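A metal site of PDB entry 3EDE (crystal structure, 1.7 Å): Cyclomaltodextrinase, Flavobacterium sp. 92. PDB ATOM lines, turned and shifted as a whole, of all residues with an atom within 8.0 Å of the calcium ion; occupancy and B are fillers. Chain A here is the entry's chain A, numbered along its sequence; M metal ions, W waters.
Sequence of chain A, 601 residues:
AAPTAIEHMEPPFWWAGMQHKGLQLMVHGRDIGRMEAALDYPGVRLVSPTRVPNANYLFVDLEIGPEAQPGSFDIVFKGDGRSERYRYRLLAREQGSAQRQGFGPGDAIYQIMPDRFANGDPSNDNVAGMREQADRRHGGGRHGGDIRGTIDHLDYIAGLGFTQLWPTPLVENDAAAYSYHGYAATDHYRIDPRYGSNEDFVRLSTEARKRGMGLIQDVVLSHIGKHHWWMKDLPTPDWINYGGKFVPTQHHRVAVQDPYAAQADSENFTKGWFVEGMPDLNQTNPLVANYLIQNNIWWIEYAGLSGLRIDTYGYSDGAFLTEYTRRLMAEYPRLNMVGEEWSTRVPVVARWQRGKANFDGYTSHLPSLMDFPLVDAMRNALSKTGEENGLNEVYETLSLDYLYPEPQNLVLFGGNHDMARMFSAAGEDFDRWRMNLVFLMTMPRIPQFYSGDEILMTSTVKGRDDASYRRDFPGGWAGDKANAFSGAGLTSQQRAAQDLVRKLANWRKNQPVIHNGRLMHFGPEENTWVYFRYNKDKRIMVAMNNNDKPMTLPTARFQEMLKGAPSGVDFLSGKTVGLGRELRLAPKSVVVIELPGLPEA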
ATOM      1  N   PRO A 114       2.190  -6.186   7.535  1.00  0.00           N
ATOM      2  CA  PRO A 114       0.846  -6.810   7.404  1.00  0.00           C
ATOM      3  C   PRO A 114       0.800  -8.191   8.092  1.00  0.00           C
ATOM      4  O   PRO A 114      -0.179  -8.482   8.756  1.00  0.00           O
ATOM      5  CB  PRO A 114       0.638  -6.929   5.892  1.00  0.00           C
ATOM      6  CG  PRO A 114       2.045  -6.680   5.273  1.00  0.00           C
ATOM      7  CD  PRO A 114       2.740  -5.776   6.215  1.00  0.00           C
ATOM      8  N   ASP A 115       1.860  -8.977   8.017  1.00  0.00           N
ATOM      9  CA  ASP A 115       1.836 -10.255   8.789  1.00  0.00           C
ATOM     10  C   ASP A 115       1.744 -10.114  10.315  1.00  0.00           C
ATOM     11  O   ASP A 115       1.329 -11.069  11.012  1.00  0.00           O
ATOM     12  CB  ASP A 115       3.065 -11.119   8.461  1.00  0.00           C
ATOM     13  CG  ASP A 115       2.973 -12.519   9.082  1.00  0.00           C
ATOM     14  OD1 ASP A 115       3.847 -12.850   9.954  1.00  0.00           O
ATOM     15  OD2 ASP A 115       1.997 -13.224   8.756  1.00  0.00           O
ATOM     16  N   ALA A 118      -2.646  -7.525  12.229  1.00  0.00           N
ATOM     17  CA  ALA A 118      -3.954  -8.096  12.607  1.00  0.00           C
ATOM     18  C   ALA A 118      -4.376  -9.253  11.715  1.00  0.00           C
ATOM     19  O   ALA A 118      -4.367  -9.153  10.499  1.00  0.00           O
ATOM     20  CB  ALA A 118      -5.046  -7.008  12.639  1.00  0.00           C
ATOM     21  N   ASN A 119      -4.723 -10.352  12.357  1.00  0.00           N
ATOM     22  CA  ASN A 119      -5.121 -11.566  11.683  1.00  0.00           C
ATOM     23  C   ASN A 119      -6.639 -11.655  11.608  1.00  0.00           C
ATOM     24  O   ASN A 119      -7.312 -12.159  12.531  1.00  0.00           O
ATOM     25  CB  ASN A 119      -4.488 -12.782  12.394  1.00  0.00           C
ATOM     26  CG  ASN A 119      -4.724 -14.095  11.635  1.00  0.00           C
ATOM     27  OD1 ASN A 119      -5.434 -14.124  10.638  1.00  0.00           O
ATOM     28  ND2 ASN A 119      -4.172 -15.194  12.160  1.00  0.00           N
ATOM     29  N   GLY A 120      -7.190 -11.069  10.545  1.00  0.00           N
ATOM     30  CA  GLY A 120      -8.636 -10.958  10.396  1.00  0.00           C
ATOM     31  C   GLY A 120      -9.264 -12.242   9.878  1.00  0.00           C
ATOM     32  O   GLY A 120     -10.482 -12.464  10.031  1.00  0.00           O
ATOM     33  N   ASP A 121      -8.431 -13.094   9.271  1.00  0.00           N
ATOM     34  CA  ASP A 121      -8.917 -14.360   8.727  1.00  0.00           C
ATOM     35  C   ASP A 121      -7.896 -15.453   9.005  1.00  0.00           C
ATOM     36  O   ASP A 121      -6.963 -15.594   8.238  1.00  0.00           O
ATOM     37  CB  ASP A 121      -9.105 -14.234   7.216  1.00  0.00           C
ATOM     38  CG  ASP A 121      -9.787 -15.455   6.623  1.00  0.00           C
ATOM     39  OD1 ASP A 121      -9.957 -16.469   7.354  1.00  0.00           O
ATOM     40  OD2 ASP A 121     -10.145 -15.384   5.439  1.00  0.00           O
ATOM     41  N   PRO A 122      -8.060 -16.226  10.092  1.00  0.00           N
ATOM     42  CA  PRO A 122      -7.068 -17.309  10.328  1.00  0.00           C
ATOM     43  C   PRO A 122      -6.989 -18.354   9.222  1.00  0.00           C
ATOM     44  O   PRO A 122      -5.966 -19.059   9.116  1.00  0.00           O
ATOM     45  CB  PRO A 122      -7.546 -17.942  11.655  1.00  0.00           C
ATOM     46  CG  PRO A 122      -8.260 -16.823  12.330  1.00  0.00           C
ATOM     47  CD  PRO A 122      -9.014 -16.148  11.212  1.00  0.00           C
ATOM     48  N   SER A 123      -8.026 -18.452   8.398  1.00  0.00           N
ATOM     49  CA  SER A 123      -8.095 -19.511   7.395  1.00  0.00           C
ATOM     50  C   SER A 123      -7.109 -19.312   6.255  1.00  0.00           C
ATOM     51  O   SER A 123      -6.809 -20.273   5.563  1.00  0.00           O
ATOM     52  CB  SER A 123      -9.502 -19.702   6.829  1.00  0.00           C
ATOM     53  OG  SER A 123      -9.861 -18.666   5.910  1.00  0.00           O
ATOM     54  N   ASN A 124      -6.610 -18.102   6.058  1.00  0.00           N
ATOM     55  CA  ASN A 124      -5.596 -17.895   5.008  1.00  0.00           C
ATOM     56  C   ASN A 124      -4.165 -17.916   5.574  1.00  0.00           C
ATOM     57  O   ASN A 124      -3.203 -17.606   4.863  1.00  0.00           O
ATOM     58  CB  ASN A 124      -5.868 -16.609   4.216  1.00  0.00           C
ATOM     59  CG  ASN A 124      -5.799 -15.365   5.069  1.00  0.00           C
ATOM     60  OD1 ASN A 124      -5.223 -15.354   6.150  1.00  0.00           O
ATOM     61  ND2 ASN A 124      -6.425 -14.293   4.586  1.00  0.00           N
ATOM     62  N   ASP A 125      -4.013 -18.278   6.849  1.00  0.00           N
ATOM     63  CA  ASP A 125      -2.672 -18.274   7.460  1.00  0.00           C
ATOM     64  C   ASP A 125      -1.767 -19.220   6.667  1.00  0.00           C
ATOM     65  O   ASP A 125      -0.578 -18.949   6.468  1.00  0.00           O
ATOM     66  CB  ASP A 125      -2.720 -18.691   8.939  1.00  0.00           C
ATOM     67  CG  ASP A 125      -3.381 -17.657   9.827  1.00  0.00           C
ATOM     68  OD1 ASP A 125      -3.834 -16.620   9.319  1.00  0.00           O
ATOM     69  OD2 ASP A 125      -3.494 -17.900  11.061  1.00  0.00           O
ATOM     70  N   ASN A 126      -2.350 -20.344   6.231  1.00  0.00           N
ATOM     71  CA  ASN A 126      -1.750 -21.269   5.263  1.00  0.00           C
ATOM     72  C   ASN A 126      -2.614 -21.308   4.027  1.00  0.00           C
ATOM     73  O   ASN A 126      -3.845 -21.193   4.097  1.00  0.00           O
ATOM     74  CB  ASN A 126      -1.638 -22.678   5.867  1.00  0.00           C
ATOM     75  CG  ASN A 126      -0.712 -22.698   7.062  1.00  0.00           C
ATOM     76  OD1 ASN A 126       0.402 -22.204   6.986  1.00  0.00           O
ATOM     77  ND2 ASN A 126      -1.180 -23.259   8.188  1.00  0.00           N
ATOM     78  N   ALA A 134       2.570 -21.456   8.573  1.00  0.00           N
ATOM     79  CA  ALA A 134       2.555 -20.434   9.601  1.00  0.00           C
ATOM     80  C   ALA A 134       3.015 -20.967  10.945  1.00  0.00           C
ATOM     81  O   ALA A 134       2.749 -22.143  11.287  1.00  0.00           O
ATOM     82  CB  ALA A 134       1.160 -19.803   9.717  1.00  0.00           C
ATOM     83  N   ARG A 142       5.693 -16.907   9.734  1.00  0.00           N
ATOM     84  CA  ARG A 142       4.428 -16.203   9.413  1.00  0.00           C
ATOM     85  C   ARG A 142       3.470 -16.311  10.593  1.00  0.00           C
ATOM     86  O   ARG A 142       3.165 -17.412  11.065  1.00  0.00           O
ATOM     87  CB  ARG A 142       3.751 -16.798   8.176  1.00  0.00           C
ATOM     88  CG  ARG A 142       4.562 -16.675   6.906  1.00  0.00           C
ATOM     89  CD  ARG A 142       3.700 -16.965   5.688  1.00  0.00           C
ATOM     90  NE  ARG A 142       2.728 -15.881   5.439  1.00  0.00           N
ATOM     91  CZ  ARG A 142       2.989 -14.811   4.690  1.00  0.00           C
ATOM     92  NH1 ARG A 142       2.055 -13.876   4.549  1.00  0.00           N
ATOM     93  NH2 ARG A 142       4.156 -14.684   4.093  1.00  0.00           N
ATOM     94  N   HIS A 143       2.990 -15.174  11.059  1.00  0.00           N
ATOM     95  CA  HIS A 143       2.059 -15.152  12.199  1.00  0.00           C
ATOM     96  C   HIS A 143       0.591 -15.112  11.819  1.00  0.00           C
ATOM     97  O   HIS A 143      -0.289 -15.512  12.623  1.00  0.00           O
ATOM     98  CB  HIS A 143       2.445 -14.016  13.160  1.00  0.00           C
ATOM     99  CG  HIS A 143       3.805 -14.177  13.758  1.00  0.00           C
ATOM    100  ND1 HIS A 143       4.298 -13.339  14.726  1.00  0.00           N
ATOM    101  CD2 HIS A 143       4.791 -15.081  13.510  1.00  0.00           C
ATOM    102  CE1 HIS A 143       5.535 -13.708  15.046  1.00  0.00           C
ATOM    103  NE2 HIS A 143       5.853 -14.762  14.311  1.00  0.00           N
ATOM    104  N   GLY A 144       0.306 -14.617  10.604  1.00  0.00           N
ATOM    105  CA  GLY A 144      -1.009 -14.724  10.027  1.00  0.00           C
ATOM    106  C   GLY A 144      -1.716 -13.399   9.834  1.00  0.00           C
ATOM    107  O   GLY A 144      -2.888 -13.380   9.471  1.00  0.00           O
ATOM    108  N   GLY A 145      -1.014 -12.285  10.052  1.00  0.00           N
ATOM    109  CA  GLY A 145      -1.674 -10.981   9.809  1.00  0.00           C
ATOM    110  C   GLY A 145      -2.102 -10.872   8.340  1.00  0.00           C
ATOM    111  O   GLY A 145      -1.444 -11.398   7.451  1.00  0.00           O
ATOM    112  N   ASP A 146      -3.177 -10.153   8.066  1.00  0.00           N
ATOM    113  CA  ASP A 146      -3.646 -10.094   6.669  1.00  0.00           C
ATOM    114  C   ASP A 146      -4.417  -8.821   6.363  1.00  0.00           C
ATOM    115  O   ASP A 146      -4.573  -7.945   7.206  1.00  0.00           O
ATOM    116  CB  ASP A 146      -4.524 -11.317   6.369  1.00  0.00           C
ATOM    117  CG  ASP A 146      -5.593 -11.537   7.460  1.00  0.00           C
ATOM    118  OD1 ASP A 146      -5.796 -12.715   7.893  1.00  0.00           O
ATOM    119  OD2 ASP A 146      -6.192 -10.534   7.907  1.00  0.00           O
ATOM    120  N   ILE A 147      -4.902  -8.729   5.120  1.00  0.00           N
ATOM    121  CA  ILE A 147      -5.600  -7.531   4.676  1.00  0.00           C
ATOM    122  C   ILE A 147      -6.933  -7.361   5.418  1.00  0.00           C
ATOM    123  O   ILE A 147      -7.314  -6.252   5.755  1.00  0.00           O
ATOM    124  CB  ILE A 147      -5.811  -7.501   3.148  1.00  0.00           C
ATOM    125  CG1 ILE A 147      -4.460  -7.319   2.449  1.00  0.00           C
ATOM    126  CG2 ILE A 147      -6.800  -6.384   2.756  1.00  0.00           C
ATOM    127  CD1 ILE A 147      -4.468  -7.636   0.958  1.00  0.00           C
ATOM    128  N   ARG A 148      -7.658  -8.453   5.634  1.00  0.00           N
ATOM    129  CA  ARG A 148      -8.872  -8.351   6.422  1.00  0.00           C
ATOM    130  C   ARG A 148      -8.653  -7.703   7.800  1.00  0.00           C
ATOM    131  O   ARG A 148      -9.422  -6.812   8.211  1.00  0.00           O
ATOM    132  CB  ARG A 148      -9.545  -9.729   6.570  1.00  0.00           C
ATOM    133  CG  ARG A 148     -10.872  -9.645   7.308  1.00  0.00           C
ATOM    134  CD  ARG A 148     -11.557 -10.980   7.263  1.00  0.00           C
ATOM    135  NE  ARG A 148     -12.747 -11.006   8.101  1.00  0.00           N
ATOM    136  CZ  ARG A 148     -13.595 -12.035   8.159  1.00  0.00           C
ATOM    137  NH1 ARG A 148     -14.648 -11.969   8.972  1.00  0.00           N
ATOM    138  NH2 ARG A 148     -13.394 -13.106   7.405  1.00  0.00           N
ATOM    139  N   GLY A 149      -7.605  -8.149   8.490  1.00  0.00           N
ATOM    140  CA  GLY A 149      -7.262  -7.613   9.821  1.00  0.00           C
ATOM    141  C   GLY A 149      -6.918  -6.130   9.713  1.00  0.00           C
ATOM    142  O   GLY A 149      -7.371  -5.312  10.534  1.00  0.00           O
ATOM    143  N   PRO A 193      -1.328 -14.825  -1.400  1.00  0.00           N
ATOM    144  CA  PRO A 193      -2.664 -15.315  -1.019  1.00  0.00           C
ATOM    145  C   PRO A 193      -2.901 -15.390   0.505  1.00  0.00           C
ATOM    146  O   PRO A 193      -4.047 -15.402   0.969  1.00  0.00           O
ATOM    147  CB  PRO A 193      -2.749 -16.724  -1.647  1.00  0.00           C
ATOM    148  CG  PRO A 193      -1.632 -16.844  -2.588  1.00  0.00           C
ATOM    149  CD  PRO A 193      -0.633 -15.724  -2.347  1.00  0.00           C
ATOM    150  N   ARG A 194      -1.820 -15.418   1.267  1.00  0.00           N
ATOM    151  CA  ARG A 194      -1.952 -15.459   2.709  1.00  0.00           C
ATOM    152  C   ARG A 194      -2.436 -14.099   3.250  1.00  0.00           C
ATOM    153  O   ARG A 194      -2.928 -14.017   4.361  1.00  0.00           O
ATOM    154  CB  ARG A 194      -0.655 -15.959   3.346  1.00  0.00           C
ATOM    155  CG  ARG A 194      -0.492 -17.447   2.979  1.00  0.00           C
ATOM    156  CD  ARG A 194       0.861 -17.947   3.267  1.00  0.00           C
ATOM    157  NE  ARG A 194       1.875 -17.292   2.425  1.00  0.00           N
ATOM    158  CZ  ARG A 194       3.095 -17.775   2.245  1.00  0.00           C
ATOM    159  NH1 ARG A 194       3.452 -18.915   2.847  1.00  0.00           N
ATOM    160  NH2 ARG A 194       3.953 -17.133   1.468  1.00  0.00           N
ATOM    161  N   TYR A 195      -2.272 -13.031   2.473  1.00  0.00           N
ATOM    162  CA  TYR A 195      -2.783 -11.735   2.881  1.00  0.00           C
ATOM    163  C   TYR A 195      -4.196 -11.491   2.354  1.00  0.00           C
ATOM    164  O   TYR A 195      -4.962 -10.739   2.969  1.00  0.00           O
ATOM    165  CB  TYR A 195      -1.853 -10.591   2.408  1.00  0.00           C
ATOM    166  CG  TYR A 195      -0.487 -10.602   3.048  1.00  0.00           C
ATOM    167  CD1 TYR A 195      -0.348 -10.654   4.433  1.00  0.00           C
ATOM    168  CD2 TYR A 195       0.677 -10.588   2.273  1.00  0.00           C
ATOM    169  CE1 TYR A 195       0.881 -10.660   5.052  1.00  0.00           C
ATOM    170  CE2 TYR A 195       1.941 -10.583   2.865  1.00  0.00           C
ATOM    171  CZ  TYR A 195       2.032 -10.658   4.270  1.00  0.00           C
ATOM    172  OH  TYR A 195       3.255 -10.654   4.910  1.00  0.00           O
ATOM    173  N   GLY A 196      -4.494 -12.084   1.206  1.00  0.00           N
ATOM    174  CA  GLY A 196      -5.761 -11.929   0.480  1.00  0.00           C
ATOM    175  C   GLY A 196      -5.538 -11.887  -1.022  1.00  0.00           C
ATOM    176  O   GLY A 196      -4.511 -12.345  -1.528  1.00  0.00           O
ATOM    177  N   TRP A 477      -4.842 -10.660  17.251  1.00  0.00           N
ATOM    178  CA  TRP A 477      -5.125 -12.103  17.193  1.00  0.00           C
ATOM    179  C   TRP A 477      -6.197 -12.436  18.207  1.00  0.00           C
ATOM    180  O   TRP A 477      -6.186 -11.906  19.324  1.00  0.00           O
ATOM    181  CB  TRP A 477      -3.879 -12.953  17.490  1.00  0.00           C
ATOM    182  CG  TRP A 477      -3.013 -13.151  16.278  1.00  0.00           C
ATOM    183  CD1 TRP A 477      -2.853 -14.314  15.556  1.00  0.00           C
ATOM    184  CD2 TRP A 477      -2.205 -12.150  15.628  1.00  0.00           C
ATOM    185  NE1 TRP A 477      -2.013 -14.083  14.472  1.00  0.00           N
ATOM    186  CE2 TRP A 477      -1.594 -12.766  14.506  1.00  0.00           C
ATOM    187  CE3 TRP A 477      -1.937 -10.795  15.893  1.00  0.00           C
ATOM    188  CZ2 TRP A 477      -0.733 -12.069  13.643  1.00  0.00           C
ATOM    189  CZ3 TRP A 477      -1.085 -10.095  15.016  1.00  0.00           C
ATOM    190  CH2 TRP A 477      -0.479 -10.738  13.918  1.00  0.00           C
HETATM  191 CA    CA M   1      -4.647 -14.682   8.348  1.00  0.00          CA
HETATM  192  O   HOH W   1      -2.494 -14.703   6.904  1.00  0.00           O
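OD1 of Asp 125 is bound to the calcium ion (2.3 Å). The side-chain carboxylate (OD1) of Asp 146 is bound to the calcium ion (2.3 Å). The calcium ion is bound by the side-chain amide oxygen (OD1) of Asn 124 (2.4 Å). O of Gly 144 binds the calcium ion, 2.5 Å away. The calcium ion is bound by OD1 of Asn 119, at 2.5 Å. The calcium ion is bound by O of Asp 121, at 2.5 Å. Water W1 binds the calcium ion (2.6 Å). The calcium ion has seven donor atoms within binding distance.
Of the 25 residues printed, 6 come within 4 Å of the calcium ion.
N of Gly 120 is in hydrogen-bond range of OD2 of Asp 146. The backbone carbonyl oxygen of Ala 118 lies within hydrogen-bond range of the backbone NH of Asp 146 (2.9 Å). The side-chain carboxylate (OD2) of Asp 146 is in hydrogen-bond range of the backbone NH (N) of Gly 149. The backbone NH of Arg 148 sits close to the side-chain carboxylate of Asp 146 (3.4 Å). O of Arg 194 sits close to OD1 of Asn 124. The backbone NH of Gly 144 lies within hydrogen-bond range of the side-chain carboxylate of Asp 115 (2.9 Å). NE1 of Trp 477 sits close to ND2 of Asn 119, 3.4 Å away. The side-chain carboxylate (OD1) of Asp 121 sits at hydrogen-bond distance from the side-chain hydroxyl (OG) of Ser 123 (2.6 Å).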
